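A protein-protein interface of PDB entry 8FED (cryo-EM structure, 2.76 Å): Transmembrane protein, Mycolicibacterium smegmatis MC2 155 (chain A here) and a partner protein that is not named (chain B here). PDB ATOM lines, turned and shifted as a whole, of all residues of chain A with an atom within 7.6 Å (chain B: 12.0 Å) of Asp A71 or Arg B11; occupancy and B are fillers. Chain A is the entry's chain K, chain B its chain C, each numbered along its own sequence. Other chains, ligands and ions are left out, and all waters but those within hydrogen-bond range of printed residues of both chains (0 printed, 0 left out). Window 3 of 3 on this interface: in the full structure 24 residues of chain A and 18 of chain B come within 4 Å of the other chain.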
ATOM      1  N   ASP A  59       4.953  -4.591  36.245  1.00  0.00           N
ATOM      2  CA  ASP A  59       5.700  -5.781  35.876  1.00  0.00           C
ATOM      3  C   ASP A  59       6.534  -6.279  37.049  1.00  0.00           C
ATOM      4  O   ASP A  59       6.498  -7.469  37.384  1.00  0.00           O
ATOM      5  CB  ASP A  59       6.593  -5.481  34.666  1.00  0.00           C
ATOM      6  CG  ASP A  59       7.121  -6.735  34.003  1.00  0.00           C
ATOM      7  OD1 ASP A  59       6.756  -7.845  34.443  1.00  0.00           O
ATOM      8  OD2 ASP A  59       7.903  -6.609  33.038  1.00  0.00           O
ATOM      9  N   PRO A  66      13.800 -10.663  35.853  1.00  0.00           N
ATOM     10  CA  PRO A  66      13.450 -10.172  34.507  1.00  0.00           C
ATOM     11  C   PRO A  66      13.016 -11.258  33.537  1.00  0.00           C
ATOM     12  O   PRO A  66      12.213 -10.978  32.637  1.00  0.00           O
ATOM     13  CB  PRO A  66      14.741  -9.483  34.042  1.00  0.00           C
ATOM     14  CG  PRO A  66      15.824 -10.095  34.867  1.00  0.00           C
ATOM     15  CD  PRO A  66      15.201 -10.366  36.199  1.00  0.00           C
ATOM     16  N   ASP A  67      13.535 -12.481  33.676  1.00  0.00           N
ATOM     17  CA  ASP A  67      13.180 -13.548  32.742  1.00  0.00           C
ATOM     18  C   ASP A  67      11.694 -13.881  32.812  1.00  0.00           C
ATOM     19  O   ASP A  67      11.048 -14.091  31.778  1.00  0.00           O
ATOM     20  CB  ASP A  67      14.025 -14.791  33.023  1.00  0.00           C
ATOM     21  CG  ASP A  67      15.504 -14.552  32.784  1.00  0.00           C
ATOM     22  OD1 ASP A  67      16.104 -13.748  33.525  1.00  0.00           O
ATOM     23  OD2 ASP A  67      16.062 -15.170  31.853  1.00  0.00           O
ATOM     24  N   ARG A  68      11.133 -13.934  34.022  1.00  0.00           N
ATOM     25  CA  ARG A  68       9.703 -14.176  34.166  1.00  0.00           C
ATOM     26  C   ARG A  68       8.865 -12.963  33.782  1.00  0.00           C
ATOM     27  O   ARG A  68       7.659 -13.106  33.555  1.00  0.00           O
ATOM     28  CB  ARG A  68       9.380 -14.602  35.599  1.00  0.00           C
ATOM     29  CG  ARG A  68      10.035 -15.906  36.024  1.00  0.00           C
ATOM     30  CD  ARG A  68       9.557 -17.070  35.171  1.00  0.00           C
ATOM     31  NE  ARG A  68      10.077 -18.347  35.646  1.00  0.00           N
ATOM     32  CZ  ARG A  68      11.242 -18.863  35.282  1.00  0.00           C
ATOM     33  NH1 ARG A  68      12.041 -18.236  34.434  1.00  0.00           N
ATOM     34  NH2 ARG A  68      11.617 -20.038  35.781  1.00  0.00           N
ATOM     35  N   ARG A  69       9.471 -11.779  33.706  1.00  0.00           N
ATOM     36  CA  ARG A  69       8.727 -10.579  33.352  1.00  0.00           C
ATOM     37  C   ARG A  69       8.368 -10.579  31.871  1.00  0.00           C
ATOM     38  O   ARG A  69       9.134 -11.051  31.026  1.00  0.00           O
ATOM     39  CB  ARG A  69       9.542  -9.331  33.688  1.00  0.00           C
ATOM     40  CG  ARG A  69       9.745  -9.100  35.176  1.00  0.00           C
ATOM     41  CD  ARG A  69      10.670  -7.923  35.434  1.00  0.00           C
ATOM     42  NE  ARG A  69      10.888  -7.706  36.859  1.00  0.00           N
ATOM     43  CZ  ARG A  69      11.763  -6.846  37.360  1.00  0.00           C
ATOM     44  NH1 ARG A  69      12.530  -6.107  36.577  1.00  0.00           N
ATOM     45  NH2 ARG A  69      11.870  -6.724  38.680  1.00  0.00           N
ATOM     46  N   ALA A  70       7.191 -10.043  31.562  1.00  0.00           N
ATOM     47  CA  ALA A  70       6.773  -9.890  30.177  1.00  0.00           C
ATOM     48  C   ALA A  70       7.550  -8.764  29.505  1.00  0.00           C
ATOM     49  O   ALA A  70       7.906  -7.761  30.131  1.00  0.00           O
ATOM     50  CB  ALA A  70       5.273  -9.615  30.096  1.00  0.00           C
ATOM     51  N   ASP A  71       7.811  -8.937  28.211  1.00  0.00           N
ATOM     52  CA  ASP A  71       8.560  -7.953  27.434  1.00  0.00           C
ATOM     53  C   ASP A  71       7.662  -6.750  27.178  1.00  0.00           C
ATOM     54  O   ASP A  71       6.845  -6.751  26.256  1.00  0.00           O
ATOM     55  CB  ASP A  71       9.049  -8.569  26.128  1.00  0.00           C
ATOM     56  CG  ASP A  71      10.022  -7.671  25.383  1.00  0.00           C
ATOM     57  OD1 ASP A  71      10.470  -6.660  25.963  1.00  0.00           O
ATOM     58  OD2 ASP A  71      10.339  -7.981  24.216  1.00  0.00           O
ATOM     59  N   LEU A  72       7.808  -5.712  28.005  1.00  0.00           N
ATOM     60  CA  LEU A  72       7.030  -4.492  27.834  1.00  0.00           C
ATOM     61  C   LEU A  72       7.541  -3.617  26.698  1.00  0.00           C
ATOM     62  O   LEU A  72       6.801  -2.745  26.229  1.00  0.00           O
ATOM     63  CB  LEU A  72       7.019  -3.682  29.133  1.00  0.00           C
ATOM     64  CG  LEU A  72       6.223  -4.263  30.300  1.00  0.00           C
ATOM     65  CD1 LEU A  72       6.350  -3.373  31.523  1.00  0.00           C
ATOM     66  CD2 LEU A  72       4.762  -4.443  29.917  1.00  0.00           C
ATOM     67  N   ALA A  73       8.783  -3.823  26.254  1.00  0.00           N
ATOM     68  CA  ALA A  73       9.332  -3.009  25.175  1.00  0.00           C
ATOM     69  C   ALA A  73       8.550  -3.196  23.882  1.00  0.00           C
ATOM     70  O   ALA A  73       8.252  -2.219  23.184  1.00  0.00           O
ATOM     71  CB  ALA A  73      10.809  -3.342  24.967  1.00  0.00           C
ATOM     72  N   MET A  74       8.204  -4.441  23.546  1.00  0.00           N
ATOM     73  CA  MET A  74       7.425  -4.694  22.337  1.00  0.00           C
ATOM     74  C   MET A  74       6.037  -4.070  22.431  1.00  0.00           C
ATOM     75  O   MET A  74       5.551  -3.469  21.463  1.00  0.00           O
ATOM     76  CB  MET A  74       7.323  -6.199  22.085  1.00  0.00           C
ATOM     77  CG  MET A  74       6.268  -6.603  21.065  1.00  0.00           C
ATOM     78  SD  MET A  74       6.502  -5.850  19.442  1.00  0.00           S
ATOM     79  CE  MET A  74       8.068  -6.559  18.954  1.00  0.00           C
ATOM     80  N   THR A  75       5.383  -4.206  23.588  1.00  0.00           N
ATOM     81  CA  THR A  75       4.054  -3.629  23.759  1.00  0.00           C
ATOM     82  C   THR A  75       4.092  -2.111  23.640  1.00  0.00           C
ATOM     83  O   THR A  75       3.224  -1.510  22.996  1.00  0.00           O
ATOM     84  CB  THR A  75       3.463  -4.041  25.106  1.00  0.00           C
ATOM     85  OG1 THR A  75       4.313  -3.583  26.165  1.00  0.00           O
ATOM     86  CG2 THR A  75       3.322  -5.554  25.187  1.00  0.00           C
ATOM     87  N   TRP A  76       5.098  -1.474  24.243  1.00  0.00           N
ATOM     88  CA  TRP A  76       5.204  -0.022  24.152  1.00  0.00           C
ATOM     89  C   TRP A  76       5.559   0.430  22.740  1.00  0.00           C
ATOM     90  O   TRP A  76       5.084   1.476  22.287  1.00  0.00           O
ATOM     91  CB  TRP A  76       6.227   0.501  25.161  1.00  0.00           C
ATOM     92  CG  TRP A  76       5.675   0.615  26.549  1.00  0.00           C
ATOM     93  CD1 TRP A  76       6.030  -0.125  27.637  1.00  0.00           C
ATOM     94  CD2 TRP A  76       4.659   1.522  26.995  1.00  0.00           C
ATOM     95  NE1 TRP A  76       5.300   0.266  28.734  1.00  0.00           N
ATOM     96  CE2 TRP A  76       4.453   1.277  28.366  1.00  0.00           C
ATOM     97  CE3 TRP A  76       3.906   2.519  26.368  1.00  0.00           C
ATOM     98  CZ2 TRP A  76       3.526   1.991  29.121  1.00  0.00           C
ATOM     99  CZ3 TRP A  76       2.987   3.226  27.119  1.00  0.00           C
ATOM    100  CH2 TRP A  76       2.805   2.960  28.481  1.00  0.00           C
ATOM    101  N   LEU A  77       6.385  -0.340  22.025  1.00  0.00           N
ATOM    102  CA  LEU A  77       6.679  -0.009  20.633  1.00  0.00           C
ATOM    103  C   LEU A  77       5.421  -0.077  19.776  1.00  0.00           C
ATOM    104  O   LEU A  77       5.159   0.819  18.964  1.00  0.00           O
ATOM    105  CB  LEU A  77       7.750  -0.949  20.081  1.00  0.00           C
ATOM    106  CG  LEU A  77       8.038  -0.792  18.588  1.00  0.00           C
ATOM    107  CD1 LEU A  77       8.772   0.511  18.317  1.00  0.00           C
ATOM    108  CD2 LEU A  77       8.822  -1.975  18.054  1.00  0.00           C
ATOM    109  N   VAL A 129       9.766   2.650  31.945  1.00  0.00           N
ATOM    110  CA  VAL A 129       9.648   1.276  32.424  1.00  0.00           C
ATOM    111  C   VAL A 129      10.913   0.853  33.162  1.00  0.00           C
ATOM    112  O   VAL A 129      10.844   0.212  34.218  1.00  0.00           O
ATOM    113  CB  VAL A 129       9.322   0.328  31.257  1.00  0.00           C
ATOM    114  CG1 VAL A 129       9.535  -1.120  31.660  1.00  0.00           C
ATOM    115  CG2 VAL A 129       7.888   0.533  30.806  1.00  0.00           C
ATOM    116  N   ARG A 133      10.924  -0.186  37.109  1.00  0.00           N
ATOM    117  CA  ARG A 133      11.447  -1.456  37.602  1.00  0.00           C
ATOM    118  C   ARG A 133      12.591  -1.243  38.586  1.00  0.00           C
ATOM    119  O   ARG A 133      12.654  -1.910  39.626  1.00  0.00           O
ATOM    120  CB  ARG A 133      11.898  -2.330  36.433  1.00  0.00           C
ATOM    121  CG  ARG A 133      10.761  -2.835  35.561  1.00  0.00           C
ATOM    122  CD  ARG A 133      11.291  -3.619  34.372  1.00  0.00           C
ATOM    123  NE  ARG A 133      10.215  -4.139  33.536  1.00  0.00           N
ATOM    124  CZ  ARG A 133      10.401  -4.751  32.375  1.00  0.00           C
ATOM    125  NH1 ARG A 133      11.612  -4.933  31.875  1.00  0.00           N
ATOM    126  NH2 ARG A 133       9.345  -5.190  31.697  1.00  0.00           N
ATOM    127  N   THR B   3      22.065 -16.964  26.028  1.00  0.00           N
ATOM    128  CA  THR B   3      21.225 -15.780  25.877  1.00  0.00           C
ATOM    129  C   THR B   3      21.041 -15.401  24.412  1.00  0.00           C
ATOM    130  O   THR B   3      19.930 -15.062  23.989  1.00  0.00           O
ATOM    131  CB  THR B   3      21.826 -14.609  26.656  1.00  0.00           C
ATOM    132  OG1 THR B   3      23.156 -14.357  26.188  1.00  0.00           O
ATOM    133  CG2 THR B   3      21.870 -14.928  28.141  1.00  0.00           C
ATOM    134  N   LEU B   4      22.120 -15.440  23.627  1.00  0.00           N
ATOM    135  CA  LEU B   4      22.026 -15.077  22.215  1.00  0.00           C
ATOM    136  C   LEU B   4      21.158 -16.061  21.440  1.00  0.00           C
ATOM    137  O   LEU B   4      20.373 -15.657  20.575  1.00  0.00           O
ATOM    138  CB  LEU B   4      23.421 -14.996  21.599  1.00  0.00           C
ATOM    139  CG  LEU B   4      24.385 -13.988  22.227  1.00  0.00           C
ATOM    140  CD1 LEU B   4      25.678 -13.913  21.433  1.00  0.00           C
ATOM    141  CD2 LEU B   4      23.735 -12.621  22.331  1.00  0.00           C
ATOM    142  N   GLN B   5      21.278 -17.356  21.742  1.00  0.00           N
ATOM    143  CA  GLN B   5      20.573 -18.406  21.016  1.00  0.00           C
ATOM    144  C   GLN B   5      19.209 -18.736  21.616  1.00  0.00           C
ATOM    145  O   GLN B   5      18.714 -19.857  21.435  1.00  0.00           O
ATOM    146  CB  GLN B   5      21.442 -19.662  20.948  1.00  0.00           C
ATOM    147  CG  GLN B   5      22.784 -19.442  20.269  1.00  0.00           C
ATOM    148  CD  GLN B   5      23.653 -20.685  20.271  1.00  0.00           C
ATOM    149  OE1 GLN B   5      23.234 -21.748  20.731  1.00  0.00           O
ATOM    150  NE2 GLN B   5      24.871 -20.556  19.757  1.00  0.00           N
ATOM    151  N   GLY B   6      18.590 -17.796  22.323  1.00  0.00           N
ATOM    152  CA  GLY B   6      17.284 -18.038  22.899  1.00  0.00           C
ATOM    153  C   GLY B   6      16.189 -18.098  21.850  1.00  0.00           C
ATOM    154  O   GLY B   6      16.355 -17.703  20.695  1.00  0.00           O
ATOM    155  N   SER B   7      15.037 -18.612  22.270  1.00  0.00           N
ATOM    156  CA  SER B   7      13.880 -18.759  21.384  1.00  0.00           C
ATOM    157  C   SER B   7      12.964 -17.538  21.447  1.00  0.00           C
ATOM    158  O   SER B   7      11.749 -17.646  21.601  1.00  0.00           O
ATOM    159  CB  SER B   7      13.120 -20.032  21.730  1.00  0.00           C
ATOM    160  OG  SER B   7      13.938 -21.176  21.559  1.00  0.00           O
ATOM    161  N   ASP B   8      13.565 -16.352  21.323  1.00  0.00           N
ATOM    162  CA  ASP B   8      12.817 -15.103  21.260  1.00  0.00           C
ATOM    163  C   ASP B   8      13.397 -14.166  20.207  1.00  0.00           C
ATOM    164  O   ASP B   8      13.149 -12.956  20.259  1.00  0.00           O
ATOM    165  CB  ASP B   8      12.797 -14.404  22.624  1.00  0.00           C
ATOM    166  CG  ASP B   8      14.176 -13.958  23.072  1.00  0.00           C
ATOM    167  OD1 ASP B   8      15.167 -14.627  22.712  1.00  0.00           O
ATOM    168  OD2 ASP B   8      14.269 -12.937  23.785  1.00  0.00           O
ATOM    169  N   ARG B   9      14.165 -14.701  19.257  1.00  0.00           N
ATOM    170  CA  ARG B   9      14.892 -13.862  18.312  1.00  0.00           C
ATOM    171  C   ARG B   9      13.976 -13.221  17.276  1.00  0.00           C
ATOM    172  O   ARG B   9      14.320 -12.173  16.723  1.00  0.00           O
ATOM    173  CB  ARG B   9      15.975 -14.687  17.618  1.00  0.00           C
ATOM    174  CG  ARG B   9      17.212 -14.956  18.462  1.00  0.00           C
ATOM    175  CD  ARG B   9      18.179 -15.858  17.711  1.00  0.00           C
ATOM    176  NE  ARG B   9      19.556 -15.697  18.162  1.00  0.00           N
ATOM    177  CZ  ARG B   9      20.609 -16.219  17.548  1.00  0.00           C
ATOM    178  NH1 ARG B   9      20.479 -16.952  16.454  1.00  0.00           N
ATOM    179  NH2 ARG B   9      21.824 -15.999  18.043  1.00  0.00           N
ATOM    180  N   PHE B  10      12.823 -13.829  16.989  1.00  0.00           N
ATOM    181  CA  PHE B  10      11.929 -13.274  15.975  1.00  0.00           C
ATOM    182  C   PHE B  10      11.314 -11.956  16.440  1.00  0.00           C
ATOM    183  O   PHE B  10      11.283 -10.970  15.690  1.00  0.00           O
ATOM    184  CB  PHE B  10      10.839 -14.290  15.628  1.00  0.00           C
ATOM    185  CG  PHE B  10       9.941 -13.858  14.504  1.00  0.00           C
ATOM    186  CD1 PHE B  10      10.310 -14.071  13.187  1.00  0.00           C
ATOM    187  CD2 PHE B  10       8.724 -13.250  14.764  1.00  0.00           C
ATOM    188  CE1 PHE B  10       9.486 -13.679  12.150  1.00  0.00           C
ATOM    189  CE2 PHE B  10       7.896 -12.855  13.730  1.00  0.00           C
ATOM    190  CZ  PHE B  10       8.278 -13.070  12.422  1.00  0.00           C
ATOM    191  N   ARG B  11      10.808 -11.928  17.675  1.00  0.00           N
ATOM    192  CA  ARG B  11      10.245 -10.699  18.223  1.00  0.00           C
ATOM    193  C   ARG B  11      11.314  -9.622  18.353  1.00  0.00           C
ATOM    194  O   ARG B  11      11.059  -8.443  18.072  1.00  0.00           O
ATOM    195  CB  ARG B  11       9.592 -10.987  19.574  1.00  0.00           C
ATOM    196  CG  ARG B  11       8.976  -9.778  20.250  1.00  0.00           C
ATOM    197  CD  ARG B  11       8.066 -10.193  21.393  1.00  0.00           C
ATOM    198  NE  ARG B  11       8.757 -11.026  22.369  1.00  0.00           N
ATOM    199  CZ  ARG B  11       8.164 -11.625  23.394  1.00  0.00           C
ATOM    200  NH1 ARG B  11       6.864 -11.507  23.606  1.00  0.00           N
ATOM    201  NH2 ARG B  11       8.895 -12.362  24.226  1.00  0.00           N
ATOM    202  N   LYS B  12      12.517 -10.013  18.779  1.00  0.00           N
ATOM    203  CA  LYS B  12      13.626  -9.068  18.859  1.00  0.00           C
ATOM    204  C   LYS B  12      13.957  -8.495  17.488  1.00  0.00           C
ATOM    205  O   LYS B  12      14.218  -7.295  17.357  1.00  0.00           O
ATOM    206  CB  LYS B  12      14.852  -9.749  19.467  1.00  0.00           C
ATOM    207  CG  LYS B  12      15.234  -9.226  20.841  1.00  0.00           C
ATOM    208  CD  LYS B  12      14.113  -9.439  21.845  1.00  0.00           C
ATOM    209  CE  LYS B  12      14.484  -8.883  23.208  1.00  0.00           C
ATOM    210  NZ  LYS B  12      13.407  -9.105  24.209  1.00  0.00           N
ATOM    211  N   GLY B  13      13.950  -9.339  16.453  1.00  0.00           N
ATOM    212  CA  GLY B  13      14.226  -8.856  15.109  1.00  0.00           C
ATOM    213  C   GLY B  13      13.175  -7.888  14.610  1.00  0.00           C
ATOM    214  O   GLY B  13      13.502  -6.853  14.025  1.00  0.00           O
ATOM    215  N   LEU B  14      11.898  -8.214  14.833  1.00  0.00           N
ATOM    216  CA  LEU B  14      10.820  -7.304  14.449  1.00  0.00           C
ATOM    217  C   LEU B  14      10.970  -5.957  15.145  1.00  0.00           C
ATOM    218  O   LEU B  14      10.941  -4.900  14.499  1.00  0.00           O
ATOM    219  CB  LEU B  14       9.463  -7.926  14.776  1.00  0.00           C
ATOM    220  CG  LEU B  14       8.633  -8.429  13.595  1.00  0.00           C
ATOM    221  CD1 LEU B  14       9.332  -9.584  12.908  1.00  0.00           C
ATOM    222  CD2 LEU B  14       7.243  -8.837  14.058  1.00  0.00           C
ATOM    223  N   MET B  15      11.147  -5.981  16.470  1.00  0.00           N
ATOM    224  CA  MET B  15      11.262  -4.740  17.226  1.00  0.00           C
ATOM    225  C   MET B  15      12.474  -3.934  16.778  1.00  0.00           C
ATOM    226  O   MET B  15      12.380  -2.717  16.581  1.00  0.00           O
ATOM    227  CB  MET B  15      11.339  -5.048  18.722  1.00  0.00           C
ATOM    228  CG  MET B  15      11.456  -3.825  19.610  1.00  0.00           C
ATOM    229  SD  MET B  15      11.037  -4.187  21.324  1.00  0.00           S
ATOM    230  CE  MET B  15      12.104  -5.588  21.646  1.00  0.00           C
ATOM    231  N   GLY B  16      13.612  -4.600  16.581  1.00  0.00           N
ATOM    232  CA  GLY B  16      14.815  -3.892  16.184  1.00  0.00           C
ATOM    233  C   GLY B  16      14.721  -3.285  14.798  1.00  0.00           C
ATOM    234  O   GLY B  16      15.162  -2.153  14.584  1.00  0.00           O
ATOM    235  N   VAL B  17      14.162  -4.023  13.835  1.00  0.00           N
ATOM    236  CA  VAL B  17      14.068  -3.484  12.483  1.00  0.00           C
ATOM    237  C   VAL B  17      13.078  -2.323  12.443  1.00  0.00           C
ATOM    238  O   VAL B  17      13.307  -1.325  11.746  1.00  0.00           O
ATOM    239  CB  VAL B  17      13.728  -4.591  11.462  1.00  0.00           C
ATOM    240  CG1 VAL B  17      12.301  -5.103  11.609  1.00  0.00           C
ATOM    241  CG2 VAL B  17      13.981  -4.100  10.044  1.00  0.00           C
ATOM    242  N   ILE B  18      11.985  -2.410  13.211  1.00  0.00           N
ATOM    243  CA  ILE B  18      11.050  -1.289  13.277  1.00  0.00           C
ATOM    244  C   ILE B  18      11.720  -0.073  13.905  1.00  0.00           C
ATOM    245  O   ILE B  18      11.559   1.058  13.427  1.00  0.00           O
ATOM    246  CB  ILE B  18       9.772  -1.699  14.033  1.00  0.00           C
ATOM    247  CG1 ILE B  18       8.980  -2.719  13.213  1.00  0.00           C
ATOM    248  CG2 ILE B  18       8.909  -0.485  14.337  1.00  0.00           C
ATOM    249  CD1 ILE B  18       7.680  -3.146  13.856  1.00  0.00           C
ATOM    250  N   VAL B  19      12.501  -0.284  14.970  1.00  0.00           N
ATOM    251  CA  VAL B  19      13.184   0.827  15.629  1.00  0.00           C
ATOM    252  C   VAL B  19      14.199   1.474  14.691  1.00  0.00           C
ATOM    253  O   VAL B  19      14.303   2.704  14.624  1.00  0.00           O
ATOM    254  CB  VAL B  19      13.837   0.349  16.940  1.00  0.00           C
ATOM    255  CG1 VAL B  19      14.852   1.364  17.441  1.00  0.00           C
ATOM    256  CG2 VAL B  19      12.774   0.116  17.997  1.00  0.00           C
ATOM    257  N   VAL B  20      14.960   0.662  13.953  1.00  0.00           N
ATOM    258  CA  VAL B  20      15.960   1.211  13.040  1.00  0.00           C
ATOM    259  C   VAL B  20      15.293   1.982  11.906  1.00  0.00           C
ATOM    260  O   VAL B  20      15.754   3.067  11.523  1.00  0.00           O
ATOM    261  CB  VAL B  20      16.878   0.093  12.512  1.00  0.00           C
ATOM    262  CG1 VAL B  20      17.781   0.617  11.409  1.00  0.00           C
ATOM    263  CG2 VAL B  20      17.721  -0.465  13.642  1.00  0.00           C
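The side-chain carboxylate (OD1) of Asp A71 lies close to the backbone NH (N) of Ala A73 (3.3 Å). The side-chain carboxylate (OD2) of Asp B8 is in salt-bridge range of the side-chain amino group (NZ) of Lys B12 (3.95 Å).
Printed residues of chain A that touch a printed residue of chain B: Asp A71, Ala A73, Met A74 and Leu A77. Along chain A the printed residues that touch a printed residue of chain B span positions 71 to 77. Hydrophobic or aromatic side chains of chain B that line the printed part of chain A: Met B15. Among the printed residues, Asp or Glu carboxylates within 4 Å of a Lys or Arg side-chain nitrogen of the other chain: Asp A71 with Arg B11 (3.9 Å) and Asp A71 with Lys B12 (3.3 Å).
No residue of chain B comes within 4 Å of Ala A70. Asp A71 touches just these residues of chain B: Arg B11 (3.9 Å), Lys B12 (3.3 Å) and Met B15 (3.9 Å). No residue of chain B comes within 4 Å of Leu A72. Met A74 touches just these residues of chain B: Arg B11 (3.6 Å) and Met B15 (3.6 Å). Printed residues of chain B within 4 Å of Leu A77: Met B15. Arg B11 touches two residues of chain A. Printed residues of chain A within 4 Å of Lys B12: Asp A71 (3.3 Å). Of the printed residues of chain A, Met B15 touches Asp A71, Ala A73, Met A74 and Leu A77. The nearest residue of chain B that does not touch Asp A71 is Asp B8 (6.3 Å). The nearest residue of chain A that does not touch Arg B11 is Ala A70 (6.5 Å).
OD2 of Asp A71 touches CE of Met B15, at 3.9 Å. C of Ala A73 touches SD of Met B15 (3.7 Å). Met A74 touches Arg B11. Leu A77 touches Met B15 (CD2 to CG, 3.6 Å).
The side-chain amino group (NZ) of Lys B12 is in salt-bridge range of the side-chain carboxylate (OD2) of Asp A71 (3.3 Å). The backbone NH (N) of Met A74 sits at hydrogen-bond distance from the side-chain sulfur (SD) of Met B15 (3.6 Å). The guanidinium group (NE) of Arg B11 lies within salt-bridge range of the side-chain carboxylate (OD2) of Asp A71, 3.9 Å away.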
